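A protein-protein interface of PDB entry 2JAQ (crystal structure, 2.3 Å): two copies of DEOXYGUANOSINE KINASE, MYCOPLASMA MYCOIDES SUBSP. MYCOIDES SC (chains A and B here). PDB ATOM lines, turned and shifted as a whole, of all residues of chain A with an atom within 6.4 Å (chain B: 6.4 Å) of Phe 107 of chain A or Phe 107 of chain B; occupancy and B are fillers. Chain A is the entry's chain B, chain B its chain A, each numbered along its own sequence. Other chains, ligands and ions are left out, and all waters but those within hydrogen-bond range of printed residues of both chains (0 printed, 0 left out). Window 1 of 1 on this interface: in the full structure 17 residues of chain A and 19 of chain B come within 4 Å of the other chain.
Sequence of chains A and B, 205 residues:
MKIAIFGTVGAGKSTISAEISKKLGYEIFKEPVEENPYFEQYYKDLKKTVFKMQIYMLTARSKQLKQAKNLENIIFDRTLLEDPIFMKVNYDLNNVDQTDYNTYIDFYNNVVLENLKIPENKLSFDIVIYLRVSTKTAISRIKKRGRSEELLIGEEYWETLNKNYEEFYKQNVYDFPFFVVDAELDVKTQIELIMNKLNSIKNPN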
ATOM      1  N   GLN A  54     -23.560  20.481  -7.890  1.00  0.00           N
ATOM      2  CA  GLN A  54     -23.429  19.183  -8.543  1.00  0.00           C
ATOM      3  C   GLN A  54     -24.174  19.082  -9.878  1.00  0.00           C
ATOM      4  O   GLN A  54     -23.757  18.332 -10.756  1.00  0.00           O
ATOM      5  CB  GLN A  54     -23.785  18.048  -7.582  1.00  0.00           C
ATOM      6  CG  GLN A  54     -22.866  17.967  -6.341  1.00  0.00           C
ATOM      7  CD  GLN A  54     -21.400  17.717  -6.684  1.00  0.00           C
ATOM      8  OE1 GLN A  54     -21.086  17.051  -7.674  1.00  0.00           O
ATOM      9  NE2 GLN A  54     -20.496  18.254  -5.866  1.00  0.00           N
ATOM     10  N   ILE A  55     -25.246  19.859 -10.042  1.00  0.00           N
ATOM     11  CA  ILE A  55     -25.929  19.973 -11.337  1.00  0.00           C
ATOM     12  C   ILE A  55     -25.070  20.781 -12.303  1.00  0.00           C
ATOM     13  O   ILE A  55     -24.911  20.416 -13.482  1.00  0.00           O
ATOM     14  CB  ILE A  55     -27.374  20.577 -11.196  1.00  0.00           C
ATOM     15  CG1 ILE A  55     -28.411  19.467 -11.017  1.00  0.00           C
ATOM     16  CG2 ILE A  55     -27.770  21.396 -12.430  1.00  0.00           C
ATOM     17  CD1 ILE A  55     -28.328  18.719  -9.705  1.00  0.00           C
ATOM     18  N   TYR A  56     -24.511  21.877 -11.798  1.00  0.00           N
ATOM     19  CA  TYR A  56     -23.554  22.652 -12.563  1.00  0.00           C
ATOM     20  C   TYR A  56     -22.394  21.778 -13.070  1.00  0.00           C
ATOM     21  O   TYR A  56     -21.969  21.904 -14.222  1.00  0.00           O
ATOM     22  CB  TYR A  56     -23.017  23.824 -11.738  1.00  0.00           C
ATOM     23  CG  TYR A  56     -21.865  24.511 -12.426  1.00  0.00           C
ATOM     24  CD1 TYR A  56     -22.093  25.529 -13.356  1.00  0.00           C
ATOM     25  CD2 TYR A  56     -20.550  24.112 -12.186  1.00  0.00           C
ATOM     26  CE1 TYR A  56     -21.028  26.148 -14.019  1.00  0.00           C
ATOM     27  CE2 TYR A  56     -19.496  24.717 -12.841  1.00  0.00           C
ATOM     28  CZ  TYR A  56     -19.739  25.736 -13.748  1.00  0.00           C
ATOM     29  OH  TYR A  56     -18.681  26.335 -14.382  1.00  0.00           O
ATOM     30  N   LEU A  58     -22.356  18.469 -13.624  1.00  0.00           N
ATOM     31  CA  LEU A  58     -22.877  17.627 -14.701  1.00  0.00           C
ATOM     32  C   LEU A  58     -22.990  18.366 -16.043  1.00  0.00           C
ATOM     33  O   LEU A  58     -22.525  17.852 -17.053  1.00  0.00           O
ATOM     34  CB  LEU A  58     -24.203  16.964 -14.305  1.00  0.00           C
ATOM     35  CG  LEU A  58     -24.168  15.929 -13.165  1.00  0.00           C
ATOM     36  CD1 LEU A  58     -25.540  15.308 -12.958  1.00  0.00           C
ATOM     37  CD2 LEU A  58     -23.132  14.820 -13.375  1.00  0.00           C
ATOM     38  N   THR A  59     -23.569  19.573 -16.030  1.00  0.00           N
ATOM     39  CA  THR A  59     -23.695  20.442 -17.222  1.00  0.00           C
ATOM     40  C   THR A  59     -22.358  20.735 -17.873  1.00  0.00           C
ATOM     41  O   THR A  59     -22.160  20.492 -19.064  1.00  0.00           O
ATOM     42  CB  THR A  59     -24.303  21.818 -16.872  1.00  0.00           C
ATOM     43  OG1 THR A  59     -25.505  21.652 -16.112  1.00  0.00           O
ATOM     44  CG2 THR A  59     -24.585  22.637 -18.146  1.00  0.00           C
ATOM     45  N   ASN A 102     -32.096  11.177  -4.712  1.00  0.00           N
ATOM     46  CA  ASN A 102     -32.887  10.481  -5.738  1.00  0.00           C
ATOM     47  C   ASN A 102     -33.024  11.309  -7.012  1.00  0.00           C
ATOM     48  O   ASN A 102     -32.817  10.797  -8.104  1.00  0.00           O
ATOM     49  CB  ASN A 102     -34.295  10.157  -5.239  1.00  0.00           C
ATOM     50  CG  ASN A 102     -34.319   9.108  -4.136  1.00  0.00           C
ATOM     51  OD1 ASN A 102     -35.312   9.001  -3.408  1.00  0.00           O
ATOM     52  ND2 ASN A 102     -33.243   8.334  -4.007  1.00  0.00           N
ATOM     53  N   THR A 103     -33.376  12.587  -6.852  1.00  0.00           N
ATOM     54  CA  THR A 103     -33.544  13.519  -7.971  1.00  0.00           C
ATOM     55  C   THR A 103     -32.312  13.527  -8.859  1.00  0.00           C
ATOM     56  O   THR A 103     -32.404  13.218 -10.043  1.00  0.00           O
ATOM     57  CB  THR A 103     -33.852  14.957  -7.479  1.00  0.00           C
ATOM     58  OG1 THR A 103     -35.091  14.948  -6.770  1.00  0.00           O
ATOM     59  CG2 THR A 103     -33.959  15.937  -8.648  1.00  0.00           C
ATOM     60  N   TYR A 104     -31.168  13.857  -8.261  1.00  0.00           N
ATOM     61  CA  TYR A 104     -29.886  13.877  -8.948  1.00  0.00           C
ATOM     62  C   TYR A 104     -29.544  12.525  -9.569  1.00  0.00           C
ATOM     63  O   TYR A 104     -29.180  12.459 -10.738  1.00  0.00           O
ATOM     64  CB  TYR A 104     -28.784  14.336  -7.981  1.00  0.00           C
ATOM     65  CG  TYR A 104     -27.372  14.198  -8.512  1.00  0.00           C
ATOM     66  CD1 TYR A 104     -26.706  15.294  -9.067  1.00  0.00           C
ATOM     67  CD2 TYR A 104     -26.695  12.978  -8.440  1.00  0.00           C
ATOM     68  CE1 TYR A 104     -25.409  15.175  -9.546  1.00  0.00           C
ATOM     69  CE2 TYR A 104     -25.397  12.847  -8.925  1.00  0.00           C
ATOM     70  CZ  TYR A 104     -24.763  13.946  -9.475  1.00  0.00           C
ATOM     71  OH  TYR A 104     -23.488  13.815  -9.953  1.00  0.00           O
ATOM     72  N   ILE A 105     -29.674  11.457  -8.786  1.00  0.00           N
ATOM     73  CA  ILE A 105     -29.300  10.113  -9.220  1.00  0.00           C
ATOM     74  C   ILE A 105     -30.098   9.649 -10.441  1.00  0.00           C
ATOM     75  O   ILE A 105     -29.524   9.166 -11.425  1.00  0.00           O
ATOM     76  CB  ILE A 105     -29.392   9.093  -8.043  1.00  0.00           C
ATOM     77  CG1 ILE A 105     -28.143   9.198  -7.154  1.00  0.00           C
ATOM     78  CG2 ILE A 105     -29.608   7.639  -8.539  1.00  0.00           C
ATOM     79  CD1 ILE A 105     -26.816   8.878  -7.858  1.00  0.00           C
ATOM     80  N   ASP A 106     -31.421   9.794 -10.362  1.00  0.00           N
ATOM     81  CA  ASP A 106     -32.309   9.497 -11.478  1.00  0.00           C
ATOM     82  C   ASP A 106     -31.982  10.433 -12.638  1.00  0.00           C
ATOM     83  O   ASP A 106     -31.859  10.017 -13.789  1.00  0.00           O
ATOM     84  CB  ASP A 106     -33.754   9.715 -11.042  1.00  0.00           C
ATOM     85  CG  ASP A 106     -34.739   9.043 -11.961  1.00  0.00           C
ATOM     86  OD1 ASP A 106     -34.439   7.911 -12.408  1.00  0.00           O
ATOM     87  OD2 ASP A 106     -35.816   9.637 -12.210  1.00  0.00           O
ATOM     88  N   PHE A 107     -31.835  11.707 -12.294  1.00  0.00           N
ATOM     89  CA  PHE A 107     -31.482  12.758 -13.226  1.00  0.00           C
ATOM     90  C   PHE A 107     -30.149  12.479 -13.925  1.00  0.00           C
ATOM     91  O   PHE A 107     -30.009  12.772 -15.109  1.00  0.00           O
ATOM     92  CB  PHE A 107     -31.466  14.095 -12.475  1.00  0.00           C
ATOM     93  CG  PHE A 107     -30.605  15.131 -13.108  1.00  0.00           C
ATOM     94  CD1 PHE A 107     -31.096  15.915 -14.137  1.00  0.00           C
ATOM     95  CD2 PHE A 107     -29.290  15.309 -12.687  1.00  0.00           C
ATOM     96  CE1 PHE A 107     -30.290  16.855 -14.738  1.00  0.00           C
ATOM     97  CE2 PHE A 107     -28.480  16.247 -13.278  1.00  0.00           C
ATOM     98  CZ  PHE A 107     -28.971  17.027 -14.302  1.00  0.00           C
ATOM     99  N   TYR A 108     -29.188  11.908 -13.191  1.00  0.00           N
ATOM    100  CA  TYR A 108     -27.881  11.524 -13.739  1.00  0.00           C
ATOM    101  C   TYR A 108     -27.983  10.421 -14.789  1.00  0.00           C
ATOM    102  O   TYR A 108     -27.271  10.449 -15.792  1.00  0.00           O
ATOM    103  CB  TYR A 108     -26.908  11.112 -12.621  1.00  0.00           C
ATOM    104  CG  TYR A 108     -25.590  10.506 -13.092  1.00  0.00           C
ATOM    105  CD1 TYR A 108     -24.616  11.290 -13.718  1.00  0.00           C
ATOM    106  CD2 TYR A 108     -25.310   9.153 -12.887  1.00  0.00           C
ATOM    107  CE1 TYR A 108     -23.406  10.742 -14.147  1.00  0.00           C
ATOM    108  CE2 TYR A 108     -24.097   8.589 -13.307  1.00  0.00           C
ATOM    109  CZ  TYR A 108     -23.151   9.388 -13.935  1.00  0.00           C
ATOM    110  OH  TYR A 108     -21.951   8.835 -14.347  1.00  0.00           O
ATOM    111  N   ASN A 109     -28.858   9.450 -14.555  1.00  0.00           N
ATOM    112  CA  ASN A 109     -29.027   8.335 -15.499  1.00  0.00           C
ATOM    113  C   ASN A 109     -30.004   8.621 -16.641  1.00  0.00           C
ATOM    114  O   ASN A 109     -29.836   8.132 -17.754  1.00  0.00           O
ATOM    115  CB  ASN A 109     -29.422   7.060 -14.760  1.00  0.00           C
ATOM    116  CG  ASN A 109     -28.337   6.581 -13.823  1.00  0.00           C
ATOM    117  OD1 ASN A 109     -27.323   6.043 -14.258  1.00  0.00           O
ATOM    118  ND2 ASN A 109     -28.538   6.786 -12.530  1.00  0.00           N
ATOM    119  N   ASN A 110     -31.016   9.431 -16.364  1.00  0.00           N
ATOM    120  CA  ASN A 110     -32.097   9.624 -17.323  1.00  0.00           C
ATOM    121  C   ASN A 110     -32.037  10.938 -18.086  1.00  0.00           C
ATOM    122  O   ASN A 110     -32.865  11.188 -18.963  1.00  0.00           O
ATOM    123  CB  ASN A 110     -33.448   9.469 -16.625  1.00  0.00           C
ATOM    124  CG  ASN A 110     -33.749   8.033 -16.250  1.00  0.00           C
ATOM    125  OD1 ASN A 110     -33.884   7.169 -17.113  1.00  0.00           O
ATOM    126  ND2 ASN A 110     -33.875   7.774 -14.954  1.00  0.00           N
ATOM    127  N   VAL A 111     -31.068  11.781 -17.743  1.00  0.00           N
ATOM    128  CA  VAL A 111     -30.890  13.063 -18.428  1.00  0.00           C
ATOM    129  C   VAL A 111     -29.445  13.228 -18.884  1.00  0.00           C
ATOM    130  O   VAL A 111     -29.185  13.419 -20.071  1.00  0.00           O
ATOM    131  CB  VAL A 111     -31.329  14.281 -17.557  1.00  0.00           C
ATOM    132  CG1 VAL A 111     -31.189  15.576 -18.342  1.00  0.00           C
ATOM    133  CG2 VAL A 111     -32.753  14.113 -17.082  1.00  0.00           C
ATOM    134  N   VAL A 112     -28.513  13.144 -17.936  1.00  0.00           N
ATOM    135  CA  VAL A 112     -27.096  13.322 -18.233  1.00  0.00           C
ATOM    136  C   VAL A 112     -26.557  12.135 -19.019  1.00  0.00           C
ATOM    137  O   VAL A 112     -26.146  12.293 -20.171  1.00  0.00           O
ATOM    138  CB  VAL A 112     -26.260  13.560 -16.962  1.00  0.00           C
ATOM    139  CG1 VAL A 112     -24.808  13.898 -17.328  1.00  0.00           C
ATOM    140  CG2 VAL A 112     -26.872  14.671 -16.137  1.00  0.00           C
ATOM    141  N   LEU A 113     -26.589  10.954 -18.404  1.00  0.00           N
ATOM    142  CA  LEU A 113     -26.052   9.743 -19.018  1.00  0.00           C
ATOM    143  C   LEU A 113     -26.737   9.459 -20.351  1.00  0.00           C
ATOM    144  O   LEU A 113     -26.063   9.258 -21.360  1.00  0.00           O
ATOM    145  CB  LEU A 113     -26.203   8.550 -18.070  1.00  0.00           C
ATOM    146  CG  LEU A 113     -25.127   7.461 -17.971  1.00  0.00           C
ATOM    147  CD1 LEU A 113     -24.904   6.706 -19.298  1.00  0.00           C
ATOM    148  CD2 LEU A 113     -23.810   8.010 -17.402  1.00  0.00           C
ATOM    149  N   GLN B  54     -37.544  22.501 -10.538  1.00  0.00           N
ATOM    150  CA  GLN B  54     -37.441  22.666 -11.984  1.00  0.00           C
ATOM    151  C   GLN B  54     -36.476  21.682 -12.654  1.00  0.00           C
ATOM    152  O   GLN B  54     -36.668  21.331 -13.813  1.00  0.00           O
ATOM    153  CB  GLN B  54     -37.148  24.121 -12.351  1.00  0.00           C
ATOM    154  CG  GLN B  54     -38.253  25.112 -11.910  1.00  0.00           C
ATOM    155  CD  GLN B  54     -39.611  24.833 -12.552  1.00  0.00           C
ATOM    156  OE1 GLN B  54     -39.690  24.354 -13.683  1.00  0.00           O
ATOM    157  NE2 GLN B  54     -40.687  25.132 -11.823  1.00  0.00           N
ATOM    158  N   ILE B  55     -35.467  21.215 -11.917  1.00  0.00           N
ATOM    159  CA  ILE B  55     -34.590  20.139 -12.396  1.00  0.00           C
ATOM    160  C   ILE B  55     -35.343  18.816 -12.386  1.00  0.00           C
ATOM    161  O   ILE B  55     -35.267  18.025 -13.344  1.00  0.00           O
ATOM    162  CB  ILE B  55     -33.251  20.052 -11.575  1.00  0.00           C
ATOM    163  CG1 ILE B  55     -32.161  20.907 -12.224  1.00  0.00           C
ATOM    164  CG2 ILE B  55     -32.730  18.614 -11.487  1.00  0.00           C
ATOM    165  CD1 ILE B  55     -32.392  22.399 -12.158  1.00  0.00           C
ATOM    166  N   TYR B  56     -36.080  18.578 -11.306  1.00  0.00           N
ATOM    167  CA  TYR B  56     -36.962  17.430 -11.236  1.00  0.00           C
ATOM    168  C   TYR B  56     -37.933  17.388 -12.428  1.00  0.00           C
ATOM    169  O   TYR B  56     -38.168  16.324 -13.010  1.00  0.00           O
ATOM    170  CB  TYR B  56     -37.738  17.417  -9.916  1.00  0.00           C
ATOM    171  CG  TYR B  56     -38.814  16.364  -9.910  1.00  0.00           C
ATOM    172  CD1 TYR B  56     -38.528  15.051  -9.525  1.00  0.00           C
ATOM    173  CD2 TYR B  56     -40.107  16.663 -10.336  1.00  0.00           C
ATOM    174  CE1 TYR B  56     -39.519  14.064  -9.548  1.00  0.00           C
ATOM    175  CE2 TYR B  56     -41.086  15.690 -10.364  1.00  0.00           C
ATOM    176  CZ  TYR B  56     -40.789  14.399  -9.964  1.00  0.00           C
ATOM    177  OH  TYR B  56     -41.778  13.445  -9.987  1.00  0.00           O
ATOM    178  N   LEU B  58     -37.570  18.756 -15.471  1.00  0.00           N
ATOM    179  CA  LEU B  58     -36.798  18.376 -16.656  1.00  0.00           C
ATOM    180  C   LEU B  58     -36.530  16.865 -16.739  1.00  0.00           C
ATOM    181  O   LEU B  58     -36.768  16.271 -17.782  1.00  0.00           O
ATOM    182  CB  LEU B  58     -35.502  19.189 -16.767  1.00  0.00           C
ATOM    183  CG  LEU B  58     -35.635  20.702 -17.021  1.00  0.00           C
ATOM    184  CD1 LEU B  58     -34.268  21.341 -17.192  1.00  0.00           C
ATOM    185  CD2 LEU B  58     -36.515  21.046 -18.228  1.00  0.00           C
ATOM    186  N   THR B  59     -36.076  16.260 -15.634  1.00  0.00           N
ATOM    187  CA  THR B  59     -35.832  14.804 -15.530  1.00  0.00           C
ATOM    188  C   THR B  59     -37.060  13.982 -15.862  1.00  0.00           C
ATOM    189  O   THR B  59     -37.032  13.110 -16.732  1.00  0.00           O
ATOM    190  CB  THR B  59     -35.421  14.389 -14.100  1.00  0.00           C
ATOM    191  OG1 THR B  59     -34.353  15.220 -13.628  1.00  0.00           O
ATOM    192  CG2 THR B  59     -35.005  12.907 -14.054  1.00  0.00           C
ATOM    193  N   ASN B 102     -28.844  31.049 -15.099  1.00  0.00           N
ATOM    194  CA  ASN B 102     -27.828  30.653 -16.087  1.00  0.00           C
ATOM    195  C   ASN B 102     -27.557  29.153 -16.056  1.00  0.00           C
ATOM    196  O   ASN B 102     -27.531  28.512 -17.097  1.00  0.00           O
ATOM    197  CB  ASN B 102     -26.501  31.373 -15.849  1.00  0.00           C
ATOM    198  CG  ASN B 102     -26.567  32.870 -16.123  1.00  0.00           C
ATOM    199  OD1 ASN B 102     -25.706  33.623 -15.654  1.00  0.00           O
ATOM    200  ND2 ASN B 102     -27.575  33.308 -16.879  1.00  0.00           N
ATOM    201  N   THR B 103     -27.358  28.613 -14.854  1.00  0.00           N
ATOM    202  CA  THR B 103     -27.087  27.185 -14.649  1.00  0.00           C
ATOM    203  C   THR B 103     -28.147  26.332 -15.327  1.00  0.00           C
ATOM    204  O   THR B 103     -27.829  25.531 -16.199  1.00  0.00           O
ATOM    205  CB  THR B 103     -27.001  26.827 -13.145  1.00  0.00           C
ATOM    206  OG1 THR B 103     -25.904  27.531 -12.563  1.00  0.00           O
ATOM    207  CG2 THR B 103     -26.788  25.324 -12.937  1.00  0.00           C
ATOM    208  N   TYR B 104     -29.402  26.543 -14.928  1.00  0.00           N
ATOM    209  CA  TYR B 104     -30.546  25.846 -15.498  1.00  0.00           C
ATOM    210  C   TYR B 104     -30.650  26.048 -17.009  1.00  0.00           C
ATOM    211  O   TYR B 104     -30.805  25.086 -17.749  1.00  0.00           O
ATOM    212  CB  TYR B 104     -31.833  26.292 -14.789  1.00  0.00           C
ATOM    213  CG  TYR B 104     -33.116  25.803 -15.426  1.00  0.00           C
ATOM    214  CD1 TYR B 104     -33.777  24.675 -14.930  1.00  0.00           C
ATOM    215  CD2 TYR B 104     -33.679  26.476 -16.515  1.00  0.00           C
ATOM    216  CE1 TYR B 104     -34.960  24.228 -15.504  1.00  0.00           C
ATOM    217  CE2 TYR B 104     -34.860  26.030 -17.102  1.00  0.00           C
ATOM    218  CZ  TYR B 104     -35.491  24.909 -16.593  1.00  0.00           C
ATOM    219  OH  TYR B 104     -36.651  24.469 -17.173  1.00  0.00           O
ATOM    220  N   ILE B 105     -30.556  27.299 -17.451  1.00  0.00           N
ATOM    221  CA  ILE B 105     -30.726  27.649 -18.859  1.00  0.00           C
ATOM    222  C   ILE B 105     -29.694  26.964 -19.760  1.00  0.00           C
ATOM    223  O   ILE B 105     -30.049  26.366 -20.784  1.00  0.00           O
ATOM    224  CB  ILE B 105     -30.740  29.194 -19.058  1.00  0.00           C
ATOM    225  CG1 ILE B 105     -32.124  29.761 -18.709  1.00  0.00           C
ATOM    226  CG2 ILE B 105     -30.309  29.607 -20.492  1.00  0.00           C
ATOM    227  CD1 ILE B 105     -33.278  29.234 -19.578  1.00  0.00           C
ATOM    228  N   ASP B 106     -28.423  27.066 -19.369  1.00  0.00           N
ATOM    229  CA  ASP B 106     -27.338  26.382 -20.056  1.00  0.00           C
ATOM    230  C   ASP B 106     -27.549  24.872 -19.955  1.00  0.00           C
ATOM    231  O   ASP B 106     -27.435  24.139 -20.937  1.00  0.00           O
ATOM    232  CB  ASP B 106     -26.012  26.758 -19.402  1.00  0.00           C
ATOM    233  CG  ASP B 106     -24.828  26.461 -20.283  1.00  0.00           C
ATOM    234  OD1 ASP B 106     -24.945  26.688 -21.512  1.00  0.00           O
ATOM    235  OD2 ASP B 106     -23.784  26.025 -19.743  1.00  0.00           O
ATOM    236  N   PHE B 107     -27.874  24.437 -18.742  1.00  0.00           N
ATOM    237  CA  PHE B 107     -28.163  23.051 -18.430  1.00  0.00           C
ATOM    238  C   PHE B 107     -29.324  22.509 -19.266  1.00  0.00           C
ATOM    239  O   PHE B 107     -29.294  21.354 -19.675  1.00  0.00           O
ATOM    240  CB  PHE B 107     -28.431  22.927 -16.924  1.00  0.00           C
ATOM    241  CG  PHE B 107     -29.280  21.760 -16.553  1.00  0.00           C
ATOM    242  CD1 PHE B 107     -28.714  20.508 -16.380  1.00  0.00           C
ATOM    243  CD2 PHE B 107     -30.655  21.912 -16.395  1.00  0.00           C
ATOM    244  CE1 PHE B 107     -29.506  19.427 -16.060  1.00  0.00           C
ATOM    245  CE2 PHE B 107     -31.450  20.840 -16.071  1.00  0.00           C
ATOM    246  CZ  PHE B 107     -30.889  19.597 -15.899  1.00  0.00           C
ATOM    247  N   TYR B 108     -30.334  23.351 -19.513  1.00  0.00           N
ATOM    248  CA  TYR B 108     -31.488  22.995 -20.348  1.00  0.00           C
ATOM    249  C   TYR B 108     -31.106  22.743 -21.803  1.00  0.00           C
ATOM    250  O   TYR B 108     -31.638  21.832 -22.437  1.00  0.00           O
ATOM    251  CB  TYR B 108     -32.592  24.062 -20.257  1.00  0.00           C
ATOM    252  CG  TYR B 108     -33.750  23.887 -21.232  1.00  0.00           C
ATOM    253  CD1 TYR B 108     -34.673  22.846 -21.081  1.00  0.00           C
ATOM    254  CD2 TYR B 108     -33.935  24.779 -22.291  1.00  0.00           C
ATOM    255  CE1 TYR B 108     -35.736  22.686 -21.972  1.00  0.00           C
ATOM    256  CE2 TYR B 108     -35.003  24.634 -23.189  1.00  0.00           C
ATOM    257  CZ  TYR B 108     -35.899  23.587 -23.022  1.00  0.00           C
ATOM    258  OH  TYR B 108     -36.954  23.443 -23.904  1.00  0.00           O
ATOM    259  N   ASN B 109     -30.199  23.554 -22.332  1.00  0.00           N
ATOM    260  CA  ASN B 109     -29.770  23.403 -23.731  1.00  0.00           C
ATOM    261  C   ASN B 109     -28.644  22.388 -23.938  1.00  0.00           C
ATOM    262  O   ASN B 109     -28.578  21.721 -24.966  1.00  0.00           O
ATOM    263  CB  ASN B 109     -29.388  24.756 -24.324  1.00  0.00           C
ATOM    264  CG  ASN B 109     -30.567  25.698 -24.406  1.00  0.00           C
ATOM    265  OD1 ASN B 109     -31.439  25.542 -25.258  1.00  0.00           O
ATOM    266  ND2 ASN B 109     -30.606  26.678 -23.512  1.00  0.00           N
ATOM    267  N   ASN B 110     -27.771  22.261 -22.947  1.00  0.00           N
ATOM    268  CA  ASN B 110     -26.567  21.457 -23.116  1.00  0.00           C
ATOM    269  C   ASN B 110     -26.618  20.093 -22.443  1.00  0.00           C
ATOM    270  O   ASN B 110     -25.682  19.302 -22.564  1.00  0.00           O
ATOM    271  CB  ASN B 110     -25.346  22.241 -22.644  1.00  0.00           C
ATOM    272  CG  ASN B 110     -24.979  23.371 -23.584  1.00  0.00           C
ATOM    273  OD1 ASN B 110     -24.618  23.143 -24.737  1.00  0.00           O
ATOM    274  ND2 ASN B 110     -25.052  24.599 -23.087  1.00  0.00           N
ATOM    275  N   VAL B 111     -27.706  19.825 -21.726  1.00  0.00           N
ATOM    276  CA  VAL B 111     -27.885  18.532 -21.060  1.00  0.00           C
ATOM    277  C   VAL B 111     -29.241  17.932 -21.412  1.00  0.00           C
ATOM    278  O   VAL B 111     -29.312  16.821 -21.933  1.00  0.00           O
ATOM    279  CB  VAL B 111     -27.714  18.619 -19.512  1.00  0.00           C
ATOM    280  CG1 VAL B 111     -27.837  17.239 -18.881  1.00  0.00           C
ATOM    281  CG2 VAL B 111     -26.383  19.237 -19.155  1.00  0.00           C
ATOM    282  N   VAL B 112     -30.307  18.680 -21.135  1.00  0.00           N
ATOM    283  CA  VAL B 112     -31.664  18.207 -21.387  1.00  0.00           C
ATOM    284  C   VAL B 112     -31.949  18.163 -22.881  1.00  0.00           C
ATOM    285  O   VAL B 112     -32.173  17.086 -23.435  1.00  0.00           O
ATOM    286  CB  VAL B 112     -32.722  19.054 -20.654  1.00  0.00           C
ATOM    287  CG1 VAL B 112     -34.115  18.431 -20.815  1.00  0.00           C
ATOM    288  CG2 VAL B 112     -32.363  19.178 -19.189  1.00  0.00           C
ATOM    289  N   LEU B 113     -31.913  19.327 -23.526  1.00  0.00           N
ATOM    290  CA  LEU B 113     -32.223  19.441 -24.948  1.00  0.00           C
ATOM    291  C   LEU B 113     -31.301  18.549 -25.776  1.00  0.00           C
ATOM    292  O   LEU B 113     -31.778  17.770 -26.601  1.00  0.00           O
ATOM    293  CB  LEU B 113     -32.125  20.898 -25.404  1.00  0.00           C
ATOM    294  CG  LEU B 113     -33.098  21.485 -26.435  1.00  0.00           C
ATOM    295  CD1 LEU B 113     -33.027  20.782 -27.805  1.00  0.00           C
ATOM    296  CD2 LEU B 113     -34.537  21.537 -25.897  1.00  0.00           C
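Of the 17 printed residues of chain A, 5 touch a printed residue of chain B. Printed residues of chain A that touch a printed residue of chain B: Thr 59, Asp 106, Phe 107, Val 111 and Val 112. Printed residues of chain B that touch a printed residue of chain A: Thr 59, Asp 106, Phe 107, Val 111 and Val 112. Hydrophobic or aromatic side chains of chain B within 4 Å of the printed part of chain A: Phe 107, Val 111 and Val 112.
The side-chain carboxylate of Asp 106 of chain A lies within hydrogen-bond range of the side-chain amide nitrogen of Asn 110 of chain A, at 2.6 Å. O of Phe 107 of chain B is in hydrogen-bond range of N of Val 112 of chain B, 3.2 Å away. OG1 of Thr 59 of chain B sits at hydrogen-bond distance from O of Ile 55 of chain B. The backbone NH of Val 112 of chain A sits at hydrogen-bond distance from the backbone carbonyl oxygen of Phe 107 of chain A (3.2 Å). O of Ile 55 of chain A is in hydrogen-bond range of OG1 of Thr 59 of chain A (3.0 Å). ND2 of Asn 110 of chain B is in hydrogen-bond range of OD1 of Asp 106 of chain B (2.6 Å).
Phe 107 of chain B touches two residues of chain A. Of the printed residues of chain A, Thr 59 of chain B touches Asp 106, Phe 107 and Val 111. Printed residues of chain B within 4 Å of Thr 59 of chain A: Asp 106 (3.8 Å), Phe 107 (3.3 Å) and Val 111 (3.5 Å). Leu 58 of chain B touches none of the printed residues of chain A. Tyr 104 of chain B touches none of the printed residues of chain A.
Among the printed residues, merely in contact across the chains: Thr 59 of chain A with Asp 106 of chain B, Thr 59 of chain A with Phe 107 of chain B, Thr 59 of chain A with Val 111 of chain B, Asp 106 of chain A with Thr 59 of chain B, Phe 107 of chain A with Thr 59 of chain B, Phe 107 of chain A with Phe 107 of chain B, Val 111 of chain A with Thr 59 of chain B, Val 111 of chain A with Val 111 of chain B, Val 111 of chain A with Val 112 of chain B and Val 112 of chain A with Val 111 of chain B.
Thr 59 of chain A touches Phe 107 of chain B, and with the chains exchanged Phe 107 of chain A touches Thr 59 of chain B. Thr 59 of chain A touches Val 111 of chain B, and with the chains exchanged Val 111 of chain A touches Thr 59 of chain B. Val 111 of chain A touches its own counterpart, Val 111 of chain B. Val 111 of chain A touches Val 112 of chain B, and with the chains exchanged Val 112 of chain A touches Val 111 of chain B.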
